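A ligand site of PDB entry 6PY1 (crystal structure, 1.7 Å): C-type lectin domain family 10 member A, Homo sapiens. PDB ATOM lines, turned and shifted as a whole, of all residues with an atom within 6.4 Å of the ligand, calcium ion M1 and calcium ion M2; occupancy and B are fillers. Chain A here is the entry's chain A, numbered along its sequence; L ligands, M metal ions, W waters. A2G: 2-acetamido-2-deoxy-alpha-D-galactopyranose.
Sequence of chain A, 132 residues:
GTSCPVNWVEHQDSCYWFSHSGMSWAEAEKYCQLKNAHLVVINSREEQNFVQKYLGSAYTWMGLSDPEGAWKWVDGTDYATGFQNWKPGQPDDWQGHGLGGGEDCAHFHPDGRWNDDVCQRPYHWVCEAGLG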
ATOM      1  N   TYR A  59      24.415 -21.025  21.018  1.00  0.00           N
ATOM      2  CA  TYR A  59      23.961 -21.723  19.803  1.00  0.00           C
ATOM      3  C   TYR A  59      22.765 -22.583  20.176  1.00  0.00           C
ATOM      4  O   TYR A  59      22.855 -23.271  21.185  1.00  0.00           O
ATOM      5  CB  TYR A  59      25.078 -22.590  19.200  1.00  0.00           C
ATOM      6  CG  TYR A  59      26.239 -21.820  18.642  1.00  0.00           C
ATOM      7  CD1 TYR A  59      26.089 -20.542  18.177  1.00  0.00           C
ATOM      8  CD2 TYR A  59      27.512 -22.353  18.689  1.00  0.00           C
ATOM      9  CE1 TYR A  59      27.184 -19.806  17.724  1.00  0.00           C
ATOM     10  CE2 TYR A  59      28.603 -21.652  18.227  1.00  0.00           C
ATOM     11  CZ  TYR A  59      28.425 -20.392  17.707  1.00  0.00           C
ATOM     12  OH  TYR A  59      29.516 -19.692  17.245  1.00  0.00           O
ATOM     13  N   ASP A  66      18.914 -31.674   7.183  1.00  0.00           N
ATOM     14  CA  ASP A  66      18.991 -32.147   5.772  1.00  0.00           C
ATOM     15  C   ASP A  66      19.753 -33.456   5.629  1.00  0.00           C
ATOM     16  O   ASP A  66      20.448 -33.615   4.633  1.00  0.00           O
ATOM     17  CB  ASP A  66      19.581 -31.068   4.877  1.00  0.00           C
ATOM     18  CG  ASP A  66      21.092 -30.920   4.952  1.00  0.00           C
ATOM     19  OD1 ASP A  66      21.667 -31.251   6.022  1.00  0.00           O
ATOM     20  OD2 ASP A  66      21.716 -30.518   3.938  1.00  0.00           O
ATOM     21  N   PRO A  67      19.620 -34.446   6.529  1.00  0.00           N
ATOM     22  CA  PRO A  67      20.483 -35.622   6.462  1.00  0.00           C
ATOM     23  C   PRO A  67      20.177 -36.512   5.236  1.00  0.00           C
ATOM     24  O   PRO A  67      21.052 -37.230   4.849  1.00  0.00           O
ATOM     25  CB  PRO A  67      20.221 -36.344   7.781  1.00  0.00           C
ATOM     26  CG  PRO A  67      18.789 -35.966   8.096  1.00  0.00           C
ATOM     27  CD  PRO A  67      18.643 -34.536   7.632  1.00  0.00           C
ATOM     28  N   GLY A  69      19.517 -35.297   2.158  1.00  0.00           N
ATOM     29  CA  GLY A  69      19.785 -34.528   0.931  1.00  0.00           C
ATOM     30  C   GLY A  69      19.172 -33.132   0.889  1.00  0.00           C
ATOM     31  O   GLY A  69      19.861 -32.222   0.403  1.00  0.00           O
ATOM     32  N   TRP A  71      16.855 -29.817   2.708  1.00  0.00           N
ATOM     33  CA  TRP A  71      16.441 -29.153   3.991  1.00  0.00           C
ATOM     34  C   TRP A  71      14.961 -29.376   4.230  1.00  0.00           C
ATOM     35  O   TRP A  71      14.142 -29.118   3.311  1.00  0.00           O
ATOM     36  CB  TRP A  71      16.796 -27.654   4.012  1.00  0.00           C
ATOM     37  CG  TRP A  71      18.263 -27.475   4.148  1.00  0.00           C
ATOM     38  CD1 TRP A  71      19.183 -27.254   3.185  1.00  0.00           C
ATOM     39  CD2 TRP A  71      18.978 -27.619   5.387  1.00  0.00           C
ATOM     40  NE1 TRP A  71      20.431 -27.220   3.733  1.00  0.00           N
ATOM     41  CE2 TRP A  71      20.344 -27.423   5.088  1.00  0.00           C
ATOM     42  CE3 TRP A  71      18.596 -27.896   6.706  1.00  0.00           C
ATOM     43  CZ2 TRP A  71      21.334 -27.547   6.057  1.00  0.00           C
ATOM     44  CZ3 TRP A  71      19.591 -27.984   7.685  1.00  0.00           C
ATOM     45  CH2 TRP A  71      20.940 -27.788   7.352  1.00  0.00           C
ATOM     46  N   LYS A  87      23.155 -17.262   8.073  1.00  0.00           N
ATOM     47  CA  LYS A  87      24.419 -16.487   8.139  1.00  0.00           C
ATOM     48  C   LYS A  87      25.011 -16.410   6.735  1.00  0.00           C
ATOM     49  O   LYS A  87      24.811 -17.298   5.913  1.00  0.00           O
ATOM     50  CB  LYS A  87      25.436 -17.190   9.037  1.00  0.00           C
ATOM     51  CG  LYS A  87      25.264 -16.966  10.520  1.00  0.00           C
ATOM     52  CD  LYS A  87      25.847 -15.633  10.983  1.00  0.00           C
ATOM     53  CE  LYS A  87      25.876 -15.476  12.495  1.00  0.00           C
ATOM     54  NZ  LYS A  87      26.182 -14.076  12.899  1.00  0.00           N
ATOM     55  N   GLY A  89      27.366 -17.151   3.876  1.00  0.00           N
ATOM     56  CA  GLY A  89      28.171 -18.331   3.531  1.00  0.00           C
ATOM     57  C   GLY A  89      27.505 -19.637   3.940  1.00  0.00           C
ATOM     58  O   GLY A  89      28.046 -20.675   3.592  1.00  0.00           O
ATOM     59  N   GLN A  90      26.393 -19.584   4.663  1.00  0.00           N
ATOM     60  CA  GLN A  90      25.674 -20.805   5.125  1.00  0.00           C
ATOM     61  C   GLN A  90      24.405 -21.020   4.308  1.00  0.00           C
ATOM     62  O   GLN A  90      23.840 -20.076   3.734  1.00  0.00           O
ATOM     63  CB  GLN A  90      25.364 -20.653   6.618  1.00  0.00           C
ATOM     64  CG  GLN A  90      26.599 -20.360   7.452  1.00  0.00           C
ATOM     65  CD  GLN A  90      27.723 -21.382   7.413  1.00  0.00           C
ATOM     66  OE1 GLN A  90      27.528 -22.537   7.121  1.00  0.00           O
ATOM     67  NE2 GLN A  90      28.914 -20.995   7.866  1.00  0.00           N
ATOM     68  N   PRO A  91      23.889 -22.261   4.208  1.00  0.00           N
ATOM     69  CA  PRO A  91      24.531 -23.463   4.741  1.00  0.00           C
ATOM     70  C   PRO A  91      25.679 -23.894   3.827  1.00  0.00           C
ATOM     71  O   PRO A  91      25.604 -23.602   2.626  1.00  0.00           O
ATOM     72  CB  PRO A  91      23.425 -24.508   4.696  1.00  0.00           C
ATOM     73  CG  PRO A  91      22.520 -24.074   3.582  1.00  0.00           C
ATOM     74  CD  PRO A  91      22.638 -22.573   3.537  1.00  0.00           C
ATOM     75  N   ASP A  92      26.697 -24.564   4.375  1.00  0.00           N
ATOM     76  CA  ASP A  92      27.895 -24.946   3.600  1.00  0.00           C
ATOM     77  C   ASP A  92      28.174 -26.443   3.685  1.00  0.00           C
ATOM     78  O   ASP A  92      29.103 -26.865   2.996  1.00  0.00           O
ATOM     79  CB  ASP A  92      29.105 -24.113   4.005  1.00  0.00           C
ATOM     80  CG  ASP A  92      29.535 -24.270   5.444  1.00  0.00           C
ATOM     81  OD1 ASP A  92      28.805 -25.011   6.171  1.00  0.00           O
ATOM     82  OD2 ASP A  92      30.550 -23.631   5.827  1.00  0.00           O
ATOM     83  N   ASP A  93      27.419 -27.236   4.462  1.00  0.00           N
ATOM     84  CA  ASP A  93      27.666 -28.682   4.604  1.00  0.00           C
ATOM     85  C   ASP A  93      29.159 -28.931   4.878  1.00  0.00           C
ATOM     86  O   ASP A  93      29.748 -29.883   4.278  1.00  0.00           O
ATOM     87  CB  ASP A  93      27.202 -29.452   3.369  1.00  0.00           C
ATOM     88  CG  ASP A  93      27.051 -30.956   3.609  1.00  0.00           C
ATOM     89  OD1 ASP A  93      26.458 -31.353   4.649  1.00  0.00           O
ATOM     90  OD2 ASP A  93      27.495 -31.733   2.732  1.00  0.00           O
ATOM     91  N   TRP A  94      29.762 -28.097   5.710  1.00  0.00           N
ATOM     92  CA  TRP A  94      31.231 -28.140   5.969  1.00  0.00           C
ATOM     93  C   TRP A  94      31.680 -29.553   6.414  1.00  0.00           C
ATOM     94  O   TRP A  94      31.054 -30.132   7.316  1.00  0.00           O
ATOM     95  CB  TRP A  94      31.637 -27.130   6.992  1.00  0.00           C
ATOM     96  CG  TRP A  94      33.098 -26.925   7.160  1.00  0.00           C
ATOM     97  CD1 TRP A  94      34.038 -26.623   6.218  1.00  0.00           C
ATOM     98  CD2 TRP A  94      33.743 -26.764   8.422  1.00  0.00           C
ATOM     99  NE1 TRP A  94      35.244 -26.369   6.807  1.00  0.00           N
ATOM    100  CE2 TRP A  94      35.084 -26.419   8.159  1.00  0.00           C
ATOM    101  CE3 TRP A  94      33.308 -26.847   9.740  1.00  0.00           C
ATOM    102  CZ2 TRP A  94      36.007 -26.235   9.188  1.00  0.00           C
ATOM    103  CZ3 TRP A  94      34.222 -26.672  10.744  1.00  0.00           C
ATOM    104  CH2 TRP A  94      35.548 -26.340  10.467  1.00  0.00           C
ATOM    105  N   GLY A 102      29.298 -34.100   6.677  1.00  0.00           N
ATOM    106  CA  GLY A 102      29.160 -32.655   6.521  1.00  0.00           C
ATOM    107  C   GLY A 102      28.418 -32.075   7.704  1.00  0.00           C
ATOM    108  O   GLY A 102      28.810 -32.360   8.839  1.00  0.00           O
ATOM    109  N   GLU A 103      27.393 -31.281   7.463  1.00  0.00           N
ATOM    110  CA  GLU A 103      26.662 -30.590   8.574  1.00  0.00           C
ATOM    111  C   GLU A 103      25.183 -30.651   8.212  1.00  0.00           C
ATOM    112  O   GLU A 103      24.814 -30.196   7.106  1.00  0.00           O
ATOM    113  CB  GLU A 103      27.152 -29.151   8.773  1.00  0.00           C
ATOM    114  CG  GLU A 103      28.587 -29.002   9.253  1.00  0.00           C
ATOM    115  CD  GLU A 103      29.084 -27.582   9.354  1.00  0.00           C
ATOM    116  OE1 GLU A 103      29.745 -27.208  10.395  1.00  0.00           O
ATOM    117  OE2 GLU A 103      28.726 -26.817   8.397  1.00  0.00           O
ATOM    118  N   ASP A 104      24.377 -31.288   9.032  1.00  0.00           N
ATOM    119  CA  ASP A 104      22.988 -31.588   8.603  1.00  0.00           C
ATOM    120  C   ASP A 104      21.919 -31.006   9.547  1.00  0.00           C
ATOM    121  O   ASP A 104      20.732 -31.338   9.341  1.00  0.00           O
ATOM    122  CB  ASP A 104      22.852 -33.102   8.446  1.00  0.00           C
ATOM    123  CG  ASP A 104      23.746 -33.713   7.385  1.00  0.00           C
ATOM    124  OD1 ASP A 104      24.251 -32.962   6.506  1.00  0.00           O
ATOM    125  OD2 ASP A 104      23.981 -34.943   7.488  1.00  0.00           O
ATOM    126  N   CYS A 105      22.248 -30.178  10.518  1.00  0.00           N
ATOM    127  CA  CYS A 105      21.265 -29.642  11.494  1.00  0.00           C
ATOM    128  C   CYS A 105      21.427 -28.122  11.624  1.00  0.00           C
ATOM    129  O   CYS A 105      22.565 -27.688  11.765  1.00  0.00           O
ATOM    130  CB  CYS A 105      21.471 -30.289  12.843  1.00  0.00           C
ATOM    131  SG  CYS A 105      20.948 -32.019  12.882  1.00  0.00           S
ATOM    132  N   HIS A 107      21.026 -24.399  13.436  1.00  0.00           N
ATOM    133  CA  HIS A 107      20.925 -23.700  14.722  1.00  0.00           C
ATOM    134  C   HIS A 107      20.970 -22.198  14.513  1.00  0.00           C
ATOM    135  O   HIS A 107      21.583 -21.734  13.536  1.00  0.00           O
ATOM    136  CB  HIS A 107      22.006 -24.178  15.717  1.00  0.00           C
ATOM    137  CG  HIS A 107      23.384 -23.746  15.332  1.00  0.00           C
ATOM    138  ND1 HIS A 107      23.936 -22.590  15.804  1.00  0.00           N
ATOM    139  CD2 HIS A 107      24.297 -24.295  14.511  1.00  0.00           C
ATOM    140  CE1 HIS A 107      25.155 -22.431  15.269  1.00  0.00           C
ATOM    141  NE2 HIS A 107      25.394 -23.442  14.460  1.00  0.00           N
ATOM    142  N   HIS A 109      22.637 -18.677  15.684  1.00  0.00           N
ATOM    143  CA  HIS A 109      23.670 -17.905  16.432  1.00  0.00           C
ATOM    144  C   HIS A 109      22.925 -16.963  17.374  1.00  0.00           C
ATOM    145  O   HIS A 109      21.734 -16.664  17.188  1.00  0.00           O
ATOM    146  CB  HIS A 109      24.504 -17.105  15.459  1.00  0.00           C
ATOM    147  CG  HIS A 109      25.554 -17.903  14.785  1.00  0.00           C
ATOM    148  ND1 HIS A 109      26.895 -17.665  14.985  1.00  0.00           N
ATOM    149  CD2 HIS A 109      25.471 -18.958  13.947  1.00  0.00           C
ATOM    150  CE1 HIS A 109      27.610 -18.512  14.265  1.00  0.00           C
ATOM    151  NE2 HIS A 109      26.758 -19.312  13.604  1.00  0.00           N
ATOM    152  N   ASN A 115      22.989 -21.317  11.017  1.00  0.00           N
ATOM    153  CA  ASN A 115      24.148 -22.074  10.543  1.00  0.00           C
ATOM    154  C   ASN A 115      23.757 -23.537  10.459  1.00  0.00           C
ATOM    155  O   ASN A 115      23.047 -24.013  11.364  1.00  0.00           O
ATOM    156  CB  ASN A 115      25.402 -21.834  11.388  1.00  0.00           C
ATOM    157  CG  ASN A 115      26.522 -22.757  11.000  1.00  0.00           C
ATOM    158  OD1 ASN A 115      26.913 -22.766   9.840  1.00  0.00           O
ATOM    159  ND2 ASN A 115      27.007 -23.595  11.937  1.00  0.00           N
ATOM    160  N   ASP A 116      24.359 -24.272   9.536  1.00  0.00           N
ATOM    161  CA  ASP A 116      24.300 -25.750   9.553  1.00  0.00           C
ATOM    162  C   ASP A 116      25.522 -26.276  10.326  1.00  0.00           C
ATOM    163  O   ASP A 116      26.662 -25.832  10.116  1.00  0.00           O
ATOM    164  CB  ASP A 116      24.146 -26.372   8.165  1.00  0.00           C
ATOM    165  CG  ASP A 116      25.264 -26.049   7.184  1.00  0.00           C
ATOM    166  OD1 ASP A 116      25.957 -24.996   7.350  1.00  0.00           O
ATOM    167  OD2 ASP A 116      25.439 -26.877   6.287  1.00  0.00           O
ATOM    168  N   ASP A 117      25.281 -27.240  11.192  1.00  0.00           N
ATOM    169  CA  ASP A 117      26.382 -27.757  12.044  1.00  0.00           C
ATOM    170  C   ASP A 117      26.195 -29.248  12.221  1.00  0.00           C
ATOM    171  O   ASP A 117      25.203 -29.829  11.747  1.00  0.00           O
ATOM    172  CB  ASP A 117      26.440 -26.974  13.387  1.00  0.00           C
ATOM    173  CG  ASP A 117      27.851 -26.821  14.001  1.00  0.00           C
ATOM    174  OD1 ASP A 117      28.664 -27.755  13.837  1.00  0.00           O
ATOM    175  OD2 ASP A 117      28.167 -25.723  14.584  1.00  0.00           O
ATOM    176  N   VAL A 118      27.144 -29.814  12.915  1.00  0.00           N
ATOM    177  CA  VAL A 118      27.179 -31.264  13.204  1.00  0.00           C
ATOM    178  C   VAL A 118      26.077 -31.565  14.219  1.00  0.00           C
ATOM    179  O   VAL A 118      26.064 -31.007  15.325  1.00  0.00           O
ATOM    180  CB  VAL A 118      28.568 -31.642  13.709  1.00  0.00           C
ATOM    181  CG1 VAL A 118      28.567 -33.066  14.239  1.00  0.00           C
ATOM    182  CG2 VAL A 118      29.616 -31.432  12.611  1.00  0.00           C
ATOM    183  N   TYR A 123      23.874 -28.494  21.863  1.00  0.00           N
ATOM    184  CA  TYR A 123      23.424 -27.107  21.813  1.00  0.00           C
ATOM    185  C   TYR A 123      22.100 -26.997  22.592  1.00  0.00           C
ATOM    186  O   TYR A 123      21.401 -28.014  22.890  1.00  0.00           O
ATOM    187  CB  TYR A 123      23.247 -26.670  20.361  1.00  0.00           C
ATOM    188  CG  TYR A 123      24.505 -26.403  19.571  1.00  0.00           C
ATOM    189  CD1 TYR A 123      25.749 -26.255  20.159  1.00  0.00           C
ATOM    190  CD2 TYR A 123      24.410 -26.282  18.183  1.00  0.00           C
ATOM    191  CE1 TYR A 123      26.882 -25.929  19.409  1.00  0.00           C
ATOM    192  CE2 TYR A 123      25.531 -25.975  17.435  1.00  0.00           C
ATOM    193  CZ  TYR A 123      26.761 -25.792  18.048  1.00  0.00           C
ATOM    194  OH  TYR A 123      27.867 -25.530  17.290  1.00  0.00           O
HETATM  195  O5  A2G L   1      32.334 -21.869   9.691  1.00  0.00           O
HETATM  196  C1  A2G L   1      31.854 -21.907  11.049  1.00  0.00           C
HETATM  197  O1  A2G L   1      32.809 -22.502  11.972  1.00  0.00           O
HETATM  198  C2  A2G L   1      30.521 -22.678  11.180  1.00  0.00           C
HETATM  199  N2  A2G L   1      30.197 -22.735  12.608  1.00  0.00           N
HETATM  200  C3  A2G L   1      30.601 -24.072  10.598  1.00  0.00           C
HETATM  201  O3  A2G L   1      29.333 -24.702  10.483  1.00  0.00           O
HETATM  202  C4  A2G L   1      31.211 -24.018   9.227  1.00  0.00           C
HETATM  203  O4  A2G L   1      30.174 -23.511   8.403  1.00  0.00           O
HETATM  204  C5  A2G L   1      32.553 -23.227   9.229  1.00  0.00           C
HETATM  205  C6  A2G L   1      33.182 -23.172   7.843  1.00  0.00           C
HETATM  206  O6  A2G L   1      34.434 -22.447   7.915  1.00  0.00           O
HETATM  207  C7  A2G L   1      29.310 -21.862  13.159  1.00  0.00           C
HETATM  208  O7  A2G L   1      28.758 -20.956  12.499  1.00  0.00           O
HETATM  209  C8  A2G L   1      28.949 -22.101  14.607  1.00  0.00           C
HETATM  210 CA    CA M   1      24.060 -31.083   5.052  1.00  0.00          CA
HETATM  211 CA    CA M   2      27.987 -24.509   8.481  1.00  0.00          CA
HETATM  212  O   HOH W   1      23.348 -33.246   3.777  1.00  0.00           O
HETATM  213  O   HOH W   2      24.225 -28.755   4.698  1.00  0.00           O
HETATM  214  O   HOH W   3      28.335 -19.123  10.670  1.00  0.00           O
HETATM  215  O   HOH W   4      24.332 -30.929   2.545  1.00  0.00           O
HETATM  216  O   HOH W   5      30.732 -25.142  14.248  1.00  0.00           O
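A ring nitrogen (NE2) of His 109 is in hydrogen-bond range of an oxygen (O7) of the ligand, at 2.8 Å.
The side-chain carboxylate (OD2) of Asp 117 lies within hydrogen-bond range of the side-chain hydroxyl (OH) of Tyr 123 (2.7 Å). O of Asp 117 is in hydrogen-bond range of N of Asp 104, at 3.2 Å. N of Asn 115 lies within hydrogen-bond range of O of His 107 (2.9 Å). The backbone carbonyl oxygen (O) of Cys 105 lies within hydrogen-bond range of the backbone NH (N) of Asp 117, at 2.8 Å. OE2 of Glu 103 sits close to N of Trp 94 (3.2 Å). The backbone NH (N) of Asp 93 sits at hydrogen-bond distance from the side-chain carboxylate (OD2) of Asp 116 (2.7 Å). OD1 of Asp 92 sits close to N of Trp 94.
Tyr 59 touches the ligand. CE3 of Trp 94 touches C4 of the ligand, 3.6 Å away. His 107 touches the ligand. Asp 117 touches the ligand. Hydrophobic or aromatic side chains within 4 Å of the ligand: Tyr 59, Trp 94, His 107 and His 109. Within 4 Å of the ligand: Tyr 59, Gln 90, Asp 92, Trp 94, Glu 103, His 107, His 109, Asn 115, Asp 116 and Asp 117.
Four residues have an atom within 4 Å of calcium ion M1: Asp 66, Asp 93, Glu 103 and Asp 104.
Five residues have an atom within 4 Å of calcium ion M2: Gln 90, Asp 92, Glu 103, Asn 115 and Asp 116. The nearest printed residue that does not touch calcium ion M2 is Asp 117 (4.7 Å).
Calcium ion M1 is bound by the backbone carbonyl oxygen (O) of Glu 103 (2.4 Å), water W2 (2.4 Å), the side-chain carboxylate (OD1) of Asp 104 (2.4 Å), the side-chain carboxylate (OD1) of Asp 93 (2.4 Å), water W4 (2.5 Å), the side-chain carboxylate (OD1) of Asp 66 (2.6 Å), water W1 (2.6 Å) and the side-chain carboxylate (OD2) of Asp 66 (2.7 Å). Calcium ion M1 has eight donor atoms within binding distance.
The side-chain carboxylate (OD1) of Asp 116 is bound to calcium ion M2, 2.4 Å away. Calcium ion M2 is bound by an oxygen (O4) of the ligand (2.4 Å). O3 of the ligand binds calcium ion M2, 2.4 Å away. OE2 of Glu 103 binds calcium ion M2, at 2.4 Å. OE1 of Gln 90 binds calcium ion M2, at 2.4 Å. The side-chain amide oxygen (OD1) of Asn 115 binds calcium ion M2 (2.5 Å). O of Asp 116 is bound to calcium ion M2, 2.5 Å away. Calcium ion M2 is bound by OD1 of Asp 92, at 2.5 Å.
Water W3 lies within hydrogen-bond range of O7 of the ligand (2.6 Å), NE2 of His 109 (3.3 Å) and NE2 of Gln 90 (3.4 Å). Water W5 bridges the side-chain carboxylate of Asp 117 (2.7 Å) and a nitrogen (N2) of the ligand (3.0 Å).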
